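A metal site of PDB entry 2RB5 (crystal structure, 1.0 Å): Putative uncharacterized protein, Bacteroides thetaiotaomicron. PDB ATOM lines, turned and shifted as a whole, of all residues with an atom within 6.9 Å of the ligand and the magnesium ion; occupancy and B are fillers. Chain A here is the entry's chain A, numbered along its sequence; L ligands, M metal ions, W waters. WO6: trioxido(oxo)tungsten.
W of the ligand is bound by OD2 of Asp 8 (2.3 Å).
The side-chain carboxylate (OD2) of Asp 215 is in hydrogen-bond range of the backbone NH (N) of Asp 211 (3.0 Å).
The side-chain hydroxyl (OG1) of Thr 12 sits at hydrogen-bond distance from the backbone NH (N) of Asp 211.
The guanidinium group of Arg 45 is in salt-bridge range of the side-chain carboxylate of Asp 10 (2.8 Å).
The side-chain carboxylate of Asp 10 is in hydrogen-bond range of the side-chain amide nitrogen of Asn 52 (3.4 Å).
NZ of Lys 188 lies within salt-bridge range of OD1 of Asp 215 (2.7 Å).
The backbone carbonyl oxygen of Ala 42 is in hydrogen-bond range of the side-chain amino group of Lys 188.
N of Asn 214 sits at hydrogen-bond distance from O of Arg 173, 2.9 Å away.
NE1 of Trp 174 lies within hydrogen-bond range of OD2 of Asp 180, 3.0 Å away.
N of Ile 9 lies close to O3 of the ligand, at 2.9 Å.
An oxygen (O3) of the ligand sits close to the side-chain hydroxyl of Thr 43 (2.8 Å).
The backbone NH (N) of Gly 44 lies close to an oxygen (O4) of the ligand (2.9 Å).
NZ of Lys 188 sits close to O4 of the ligand, 3.0 Å away.
An oxygen (O4) of the ligand lies close to the side-chain amide nitrogen (ND2) of Asn 214 (3.0 Å).
Residues that only touch the ligand: Trp 174 (3.0 Å).
Hydrophobic or aromatic side chains within 4 Å of the ligand: Ile 9 and Trp 174.
Of the 26 residues printed, 8 come within 4 Å of the ligand.
The nearest printed residue that does not touch the ligand is Arg 45 (4.03 Å).
Merely in contact with the magnesium ion: Asp 215.
Within 4 Å of the magnesium ion: Asp 8, Asp 10, Asp 211 and Asp 215.
The magnesium ion is bound by the side-chain carboxylate (OD1) of Asp 211 (2.1 Å), water W2 (2.1 Å), the side-chain carboxylate (OD1) of Asp 8 (2.1 Å), an oxygen (O2) of the ligand (2.1 Å), the backbone carbonyl oxygen (O) of Asp 10 (2.1 Å) and water W1 (2.1 Å).
The magnesium ion has six donor atoms within binding distance.
Water W1 lies within hydrogen-bond range of OD2 of Asp 215, OD1 of Asn 214 and N of Gly 212.
Water W2 lies within hydrogen-bond range of O of Trp 174 (2.7 Å) and OD2 of Asp 211 (2.8 Å).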
ATOM      1  N   PHE A   7      21.987   2.544   4.528  1.00  0.00           N
ATOM      2  CA  PHE A   7      21.465   1.204   4.750  1.00  0.00           C
ATOM      3  C   PHE A   7      20.181   0.948   3.975  1.00  0.00           C
ATOM      4  O   PHE A   7      19.177   1.625   4.182  1.00  0.00           O
ATOM      5  CB  PHE A   7      21.114   0.985   6.219  1.00  0.00           C
ATOM      6  CG  PHE A   7      22.286   1.011   7.159  1.00  0.00           C
ATOM      7  CD1 PHE A   7      22.603   2.162   7.869  1.00  0.00           C
ATOM      8  CD2 PHE A   7      23.078  -0.109   7.342  1.00  0.00           C
ATOM      9  CE1 PHE A   7      23.692   2.184   8.723  1.00  0.00           C
ATOM     10  CE2 PHE A   7      24.166  -0.077   8.196  1.00  0.00           C
ATOM     11  CZ  PHE A   7      24.483   1.066   8.886  1.00  0.00           C
ATOM     12  N   ASP A   8      20.210  -0.092   3.123  1.00  0.00           N
ATOM     13  CA  ASP A   8      18.955  -0.705   2.681  1.00  0.00           C
ATOM     14  C   ASP A   8      18.202  -1.223   3.923  1.00  0.00           C
ATOM     15  O   ASP A   8      18.796  -1.510   4.965  1.00  0.00           O
ATOM     16  CB  ASP A   8      19.308  -1.819   1.721  1.00  0.00           C
ATOM     17  CG  ASP A   8      18.111  -2.615   1.258  1.00  0.00           C
ATOM     18  OD1 ASP A   8      18.129  -3.849   1.420  1.00  0.00           O
ATOM     19  OD2 ASP A   8      17.179  -1.955   0.729  1.00  0.00           O
ATOM     20  N   ILE A   9      16.872  -1.364   3.767  1.00  0.00           N
ATOM     21  CA  ILE A   9      16.077  -1.929   4.859  1.00  0.00           C
ATOM     22  C   ILE A   9      15.950  -3.443   4.714  1.00  0.00           C
ATOM     23  O   ILE A   9      16.512  -4.214   5.525  1.00  0.00           O
ATOM     24  CB  ILE A   9      14.672  -1.297   4.982  1.00  0.00           C
ATOM     25  CG1 ILE A   9      14.750   0.230   5.169  1.00  0.00           C
ATOM     26  CG2 ILE A   9      13.948  -1.939   6.137  1.00  0.00           C
ATOM     27  CD1 ILE A   9      13.391   0.909   5.062  1.00  0.00           C
ATOM     28  N   ASP A  10      15.194  -3.920   3.754  1.00  0.00           N
ATOM     29  CA  ASP A  10      14.788  -5.326   3.717  1.00  0.00           C
ATOM     30  C   ASP A  10      15.935  -6.210   3.314  1.00  0.00           C
ATOM     31  O   ASP A  10      16.554  -6.078   2.280  1.00  0.00           O
ATOM     32  CB  ASP A  10      13.628  -5.480   2.751  1.00  0.00           C
ATOM     33  CG  ASP A  10      12.457  -4.641   3.203  1.00  0.00           C
ATOM     34  OD1 ASP A  10      11.818  -4.995   4.198  1.00  0.00           O
ATOM     35  OD2 ASP A  10      12.221  -3.545   2.563  1.00  0.00           O
ATOM     36  N   GLY A  11      16.258  -7.161   4.227  1.00  0.00           N
ATOM     37  CA  GLY A  11      17.393  -8.046   4.014  1.00  0.00           C
ATOM     38  C   GLY A  11      18.732  -7.476   4.451  1.00  0.00           C
ATOM     39  O   GLY A  11      19.741  -8.167   4.343  1.00  0.00           O
ATOM     40  N   THR A  12      18.749  -6.240   4.919  1.00  0.00           N
ATOM     41  CA  THR A  12      19.961  -5.519   5.318  1.00  0.00           C
ATOM     42  C   THR A  12      19.877  -5.088   6.765  1.00  0.00           C
ATOM     43  O   THR A  12      20.718  -5.530   7.578  1.00  0.00           O
ATOM     44  CB  THR A  12      20.209  -4.368   4.318  1.00  0.00           C
ATOM     45  OG1 THR A  12      20.361  -4.920   3.003  1.00  0.00           O
ATOM     46  CG2 THR A  12      21.457  -3.613   4.707  1.00  0.00           C
ATOM     47  N   PHE A  16      14.270 -10.829   6.502  1.00  0.00           N
ATOM     48  CA  PHE A  16      13.074 -11.397   5.888  1.00  0.00           C
ATOM     49  C   PHE A  16      12.563 -12.613   6.677  1.00  0.00           C
ATOM     50  O   PHE A  16      11.379 -12.985   6.583  1.00  0.00           O
ATOM     51  CB  PHE A  16      13.369 -11.818   4.453  1.00  0.00           C
ATOM     52  CG  PHE A  16      13.471 -10.739   3.396  1.00  0.00           C
ATOM     53  CD1 PHE A  16      12.368 -10.039   2.957  1.00  0.00           C
ATOM     54  CD2 PHE A  16      14.722 -10.408   2.833  1.00  0.00           C
ATOM     55  CE1 PHE A  16      12.454  -9.075   1.976  1.00  0.00           C
ATOM     56  CE2 PHE A  16      14.757  -9.448   1.824  1.00  0.00           C
ATOM     57  CZ  PHE A  16      13.675  -8.765   1.364  1.00  0.00           C
ATOM     58  N   ILE A  41      18.796   5.897   5.700  1.00  0.00           N
ATOM     59  CA  ILE A  41      18.053   4.811   5.072  1.00  0.00           C
ATOM     60  C   ILE A  41      18.082   5.011   3.556  1.00  0.00           C
ATOM     61  O   ILE A  41      17.931   6.147   3.085  1.00  0.00           O
ATOM     62  CB  ILE A  41      16.617   4.814   5.628  1.00  0.00           C
ATOM     63  CG1 ILE A  41      16.631   4.588   7.140  1.00  0.00           C
ATOM     64  CG2 ILE A  41      15.714   3.870   4.863  1.00  0.00           C
ATOM     65  CD1 ILE A  41      17.222   3.265   7.573  1.00  0.00           C
ATOM     66  N   ALA A  42      18.261   3.920   2.806  1.00  0.00           N
ATOM     67  CA  ALA A  42      18.239   3.951   1.356  1.00  0.00           C
ATOM     68  C   ALA A  42      17.400   2.787   0.889  1.00  0.00           C
ATOM     69  O   ALA A  42      17.922   1.644   0.812  1.00  0.00           O
ATOM     70  CB  ALA A  42      19.654   3.955   0.801  1.00  0.00           C
ATOM     71  N   THR A  43      16.145   3.034   0.556  1.00  0.00           N
ATOM     72  CA  THR A  43      15.174   1.985   0.341  1.00  0.00           C
ATOM     73  C   THR A  43      14.335   2.219  -0.913  1.00  0.00           C
ATOM     74  O   THR A  43      14.086   3.343  -1.340  1.00  0.00           O
ATOM     75  CB  THR A  43      14.240   1.881   1.601  1.00  0.00           C
ATOM     76  OG1 THR A  43      13.325   0.794   1.442  1.00  0.00           O
ATOM     77  CG2 THR A  43      13.413   3.116   1.846  1.00  0.00           C
ATOM     78  N   GLY A  44      13.908   1.102  -1.526  1.00  0.00           N
ATOM     79  CA  GLY A  44      12.911   1.116  -2.523  1.00  0.00           C
ATOM     80  C   GLY A  44      11.517   1.396  -1.986  1.00  0.00           C
ATOM     81  O   GLY A  44      10.625   1.752  -2.761  1.00  0.00           O
ATOM     82  N   ARG A  45      11.277   1.198  -0.711  1.00  0.00           N
ATOM     83  CA  ARG A  45       9.985   1.476  -0.149  1.00  0.00           C
ATOM     84  C   ARG A  45       9.673   2.969  -0.226  1.00  0.00           C
ATOM     85  O   ARG A  45      10.551   3.783   0.093  1.00  0.00           O
ATOM     86  CB  ARG A  45       9.895   1.051   1.319  1.00  0.00           C
ATOM     87  CG  ARG A  45       9.963  -0.453   1.546  1.00  0.00           C
ATOM     88  CD  ARG A  45       9.854  -0.779   3.019  1.00  0.00           C
ATOM     89  NE  ARG A  45       9.886  -2.199   3.303  1.00  0.00           N
ATOM     90  CZ  ARG A  45       8.922  -2.895   3.875  1.00  0.00           C
ATOM     91  NH1 ARG A  45       7.777  -2.360   4.233  1.00  0.00           N
ATOM     92  NH2 ARG A  45       9.119  -4.185   4.107  1.00  0.00           N
ATOM     93  N   ASN A  52       8.639  -0.774   9.508  1.00  0.00           N
ATOM     94  CA  ASN A  52       9.548  -1.782  10.102  1.00  0.00           C
ATOM     95  C   ASN A  52      10.781  -1.191  10.714  1.00  0.00           C
ATOM     96  O   ASN A  52      11.685  -1.955  11.049  1.00  0.00           O
ATOM     97  CB  ASN A  52       9.845  -2.869   9.086  1.00  0.00           C
ATOM     98  CG  ASN A  52      10.456  -2.361   7.779  1.00  0.00           C
ATOM     99  OD1 ASN A  52      10.663  -1.166   7.614  1.00  0.00           O
ATOM    100  ND2 ASN A  52      10.726  -3.317   6.911  1.00  0.00           N
ATOM    101  N   ASN A  69      13.847   4.415  -4.096  1.00  0.00           N
ATOM    102  CA  ASN A  69      15.043   4.191  -4.912  1.00  0.00           C
ATOM    103  C   ASN A  69      15.744   5.477  -5.325  1.00  0.00           C
ATOM    104  O   ASN A  69      16.412   5.513  -6.356  1.00  0.00           O
ATOM    105  CB  ASN A  69      14.738   3.317  -6.131  1.00  0.00           C
ATOM    106  CG  ASN A  69      14.359   1.932  -5.717  1.00  0.00           C
ATOM    107  OD1 ASN A  69      15.209   1.166  -5.250  1.00  0.00           O
ATOM    108  ND2 ASN A  69      13.039   1.617  -5.812  1.00  0.00           N
ATOM    109  N   ARG A 173      15.067  -4.345  -8.545  1.00  0.00           N
ATOM    110  CA  ARG A 173      14.350  -5.256  -7.623  1.00  0.00           C
ATOM    111  C   ARG A 173      15.082  -5.394  -6.280  1.00  0.00           C
ATOM    112  O   ARG A 173      16.301  -5.590  -6.224  1.00  0.00           O
ATOM    113  CB  ARG A 173      14.202  -6.648  -8.212  1.00  0.00           C
ATOM    114  CG  ARG A 173      13.554  -6.671  -9.607  1.00  0.00           C
ATOM    115  CD  ARG A 173      13.196  -8.110 -10.068  1.00  0.00           C
ATOM    116  NE  ARG A 173      12.538  -7.989 -11.346  1.00  0.00           N
ATOM    117  CZ  ARG A 173      11.329  -8.319 -11.707  1.00  0.00           C
ATOM    118  NH1 ARG A 173      10.498  -8.934 -10.886  1.00  0.00           N
ATOM    119  NH2 ARG A 173      10.913  -8.084 -12.970  1.00  0.00           N
ATOM    120  N   TRP A 174      14.262  -5.407  -5.211  1.00  0.00           N
ATOM    121  CA  TRP A 174      14.700  -5.843  -3.899  1.00  0.00           C
ATOM    122  C   TRP A 174      14.032  -7.120  -3.416  1.00  0.00           C
ATOM    123  O   TRP A 174      14.349  -7.646  -2.353  1.00  0.00           O
ATOM    124  CB  TRP A 174      14.395  -4.787  -2.904  1.00  0.00           C
ATOM    125  CG  TRP A 174      13.061  -4.149  -2.754  1.00  0.00           C
ATOM    126  CD1 TRP A 174      12.595  -3.109  -3.516  1.00  0.00           C
ATOM    127  CD2 TRP A 174      12.013  -4.450  -1.808  1.00  0.00           C
ATOM    128  NE1 TRP A 174      11.358  -2.737  -3.102  1.00  0.00           N
ATOM    129  CE2 TRP A 174      11.008  -3.549  -2.052  1.00  0.00           C
ATOM    130  CE3 TRP A 174      11.925  -5.376  -0.775  1.00  0.00           C
ATOM    131  CZ2 TRP A 174       9.861  -3.546  -1.318  1.00  0.00           C
ATOM    132  CZ3 TRP A 174      10.780  -5.384  -0.012  1.00  0.00           C
ATOM    133  CH2 TRP A 174       9.730  -4.436  -0.291  1.00  0.00           C
ATOM    134  N   TYR A 175      13.114  -7.639  -4.251  1.00  0.00           N
ATOM    135  CA  TYR A 175      12.413  -8.868  -3.965  1.00  0.00           C
ATOM    136  C   TYR A 175      12.077  -9.486  -5.312  1.00  0.00           C
ATOM    137  O   TYR A 175      11.793  -8.732  -6.246  1.00  0.00           O
ATOM    138  CB  TYR A 175      11.162  -8.590  -3.124  1.00  0.00           C
ATOM    139  CG  TYR A 175      10.618  -9.868  -2.557  1.00  0.00           C
ATOM    140  CD1 TYR A 175      11.180 -10.532  -1.491  1.00  0.00           C
ATOM    141  CD2 TYR A 175       9.487 -10.453  -3.105  1.00  0.00           C
ATOM    142  CE1 TYR A 175      10.664 -11.715  -0.972  1.00  0.00           C
ATOM    143  CE2 TYR A 175       8.929 -11.628  -2.633  1.00  0.00           C
ATOM    144  CZ  TYR A 175       9.556 -12.245  -1.557  1.00  0.00           C
ATOM    145  OH  TYR A 175       8.987 -13.411  -1.085  1.00  0.00           O
ATOM    146  N   PHE A 178       8.428  -8.615  -7.842  1.00  0.00           N
ATOM    147  CA  PHE A 178       8.016  -7.319  -8.404  1.00  0.00           C
ATOM    148  C   PHE A 178       9.250  -6.474  -8.631  1.00  0.00           C
ATOM    149  O   PHE A 178      10.327  -6.787  -8.133  1.00  0.00           O
ATOM    150  CB  PHE A 178       7.048  -6.688  -7.419  1.00  0.00           C
ATOM    151  CG  PHE A 178       7.545  -6.460  -6.008  1.00  0.00           C
ATOM    152  CD1 PHE A 178       8.227  -5.293  -5.694  1.00  0.00           C
ATOM    153  CD2 PHE A 178       7.344  -7.348  -4.958  1.00  0.00           C
ATOM    154  CE1 PHE A 178       8.718  -5.050  -4.403  1.00  0.00           C
ATOM    155  CE2 PHE A 178       7.873  -7.199  -3.712  1.00  0.00           C
ATOM    156  CZ  PHE A 178       8.591  -6.025  -3.470  1.00  0.00           C
ATOM    157  N   ASP A 180      10.553  -2.104  -8.989  1.00  0.00           N
ATOM    158  CA  ASP A 180      10.291  -0.709  -8.822  1.00  0.00           C
ATOM    159  C   ASP A 180      10.818   0.077 -10.022  1.00  0.00           C
ATOM    160  O   ASP A 180      11.965  -0.103 -10.433  1.00  0.00           O
ATOM    161  CB  ASP A 180      10.969  -0.143  -7.584  1.00  0.00           C
ATOM    162  CG  ASP A 180      10.504  -0.697  -6.276  1.00  0.00           C
ATOM    163  OD1 ASP A 180       9.285  -1.015  -6.115  1.00  0.00           O
ATOM    164  OD2 ASP A 180      11.373  -0.761  -5.346  1.00  0.00           O
ATOM    165  N   LYS A 188      19.460   4.433  -6.003  1.00  0.00           N
ATOM    166  CA  LYS A 188      19.989   4.819  -4.676  1.00  0.00           C
ATOM    167  C   LYS A 188      21.286   5.585  -4.799  1.00  0.00           C
ATOM    168  O   LYS A 188      21.609   6.355  -3.886  1.00  0.00           O
ATOM    169  CB  LYS A 188      20.136   3.601  -3.787  1.00  0.00           C
ATOM    170  CG  LYS A 188      18.808   2.941  -3.427  1.00  0.00           C
ATOM    171  CD  LYS A 188      18.975   1.707  -2.580  1.00  0.00           C
ATOM    172  CE  LYS A 188      17.675   0.980  -2.434  1.00  0.00           C
ATOM    173  NZ  LYS A 188      17.745  -0.130  -1.437  1.00  0.00           N
ATOM    174  N   GLY A 210      23.858  -3.369   1.523  1.00  0.00           N
ATOM    175  CA  GLY A 210      22.703  -3.878   0.811  1.00  0.00           C
ATOM    176  C   GLY A 210      22.757  -5.348   0.550  1.00  0.00           C
ATOM    177  O   GLY A 210      23.803  -5.998   0.683  1.00  0.00           O
ATOM    178  N   ASP A 211      21.605  -5.871   0.127  1.00  0.00           N
ATOM    179  CA  ASP A 211      21.411  -7.273  -0.160  1.00  0.00           C
ATOM    180  C   ASP A 211      20.827  -7.541  -1.559  1.00  0.00           C
ATOM    181  O   ASP A 211      20.760  -8.727  -1.902  1.00  0.00           O
ATOM    182  CB  ASP A 211      20.495  -7.976   0.841  1.00  0.00           C
ATOM    183  CG  ASP A 211      19.052  -7.594   0.653  1.00  0.00           C
ATOM    184  OD1 ASP A 211      18.803  -6.363   0.501  1.00  0.00           O
ATOM    185  OD2 ASP A 211      18.172  -8.490   0.581  1.00  0.00           O
ATOM    186  N   GLY A 212      20.399  -6.551  -2.255  1.00  0.00           N
ATOM    187  CA  GLY A 212      19.527  -6.767  -3.438  1.00  0.00           C
ATOM    188  C   GLY A 212      20.035  -6.111  -4.684  1.00  0.00           C
ATOM    189  O   GLY A 212      20.935  -5.257  -4.725  1.00  0.00           O
ATOM    190  N   GLY A 213      19.391  -6.468  -5.813  1.00  0.00           N
ATOM    191  CA  GLY A 213      19.776  -5.903  -7.087  1.00  0.00           C
ATOM    192  C   GLY A 213      19.615  -4.397  -7.140  1.00  0.00           C
ATOM    193  O   GLY A 213      20.434  -3.710  -7.827  1.00  0.00           O
ATOM    194  N   ASN A 214      18.652  -3.832  -6.439  1.00  0.00           N
ATOM    195  CA  ASN A 214      18.450  -2.385  -6.393  1.00  0.00           C
ATOM    196  C   ASN A 214      19.461  -1.659  -5.503  1.00  0.00           C
ATOM    197  O   ASN A 214      19.404  -0.451  -5.425  1.00  0.00           O
ATOM    198  CB  ASN A 214      17.009  -2.001  -6.020  1.00  0.00           C
ATOM    199  CG  ASN A 214      16.669  -2.238  -4.572  1.00  0.00           C
ATOM    200  OD1 ASN A 214      17.240  -3.161  -3.929  1.00  0.00           O
ATOM    201  ND2 ASN A 214      15.727  -1.441  -4.032  1.00  0.00           N
ATOM    202  N   ASP A 215      20.406  -2.432  -4.911  1.00  0.00           N
ATOM    203  CA  ASP A 215      21.507  -1.861  -4.142  1.00  0.00           C
ATOM    204  C   ASP A 215      22.797  -1.815  -4.960  1.00  0.00           C
ATOM    205  O   ASP A 215      23.761  -1.212  -4.505  1.00  0.00           O
ATOM    206  CB  ASP A 215      21.761  -2.685  -2.879  1.00  0.00           C
ATOM    207  CG  ASP A 215      20.540  -2.679  -1.972  1.00  0.00           C
ATOM    208  OD1 ASP A 215      19.965  -1.576  -1.805  1.00  0.00           O
ATOM    209  OD2 ASP A 215      20.217  -3.773  -1.447  1.00  0.00           O
HETATM  210  W   WO6 L   1      14.956  -2.321   0.332  1.00  0.00           W
HETATM  211  O1  WO6 L   1      13.152  -2.466   0.126  1.00  0.00           O
HETATM  212  O2  WO6 L   1      15.425  -3.997   0.363  1.00  0.00           O
HETATM  213  O3  WO6 L   1      14.815  -1.514   1.799  1.00  0.00           O
HETATM  214  O4  WO6 L   1      15.124  -1.458  -1.099  1.00  0.00           O
HETATM  215 MG    MG M   1      17.045  -5.301   0.410  1.00  0.00          MG
HETATM  216  O   HOH W   1      17.687  -4.522  -1.437  1.00  0.00           O
HETATM  217  O   HOH W   2      16.087  -6.932  -0.404  1.00  0.00           O
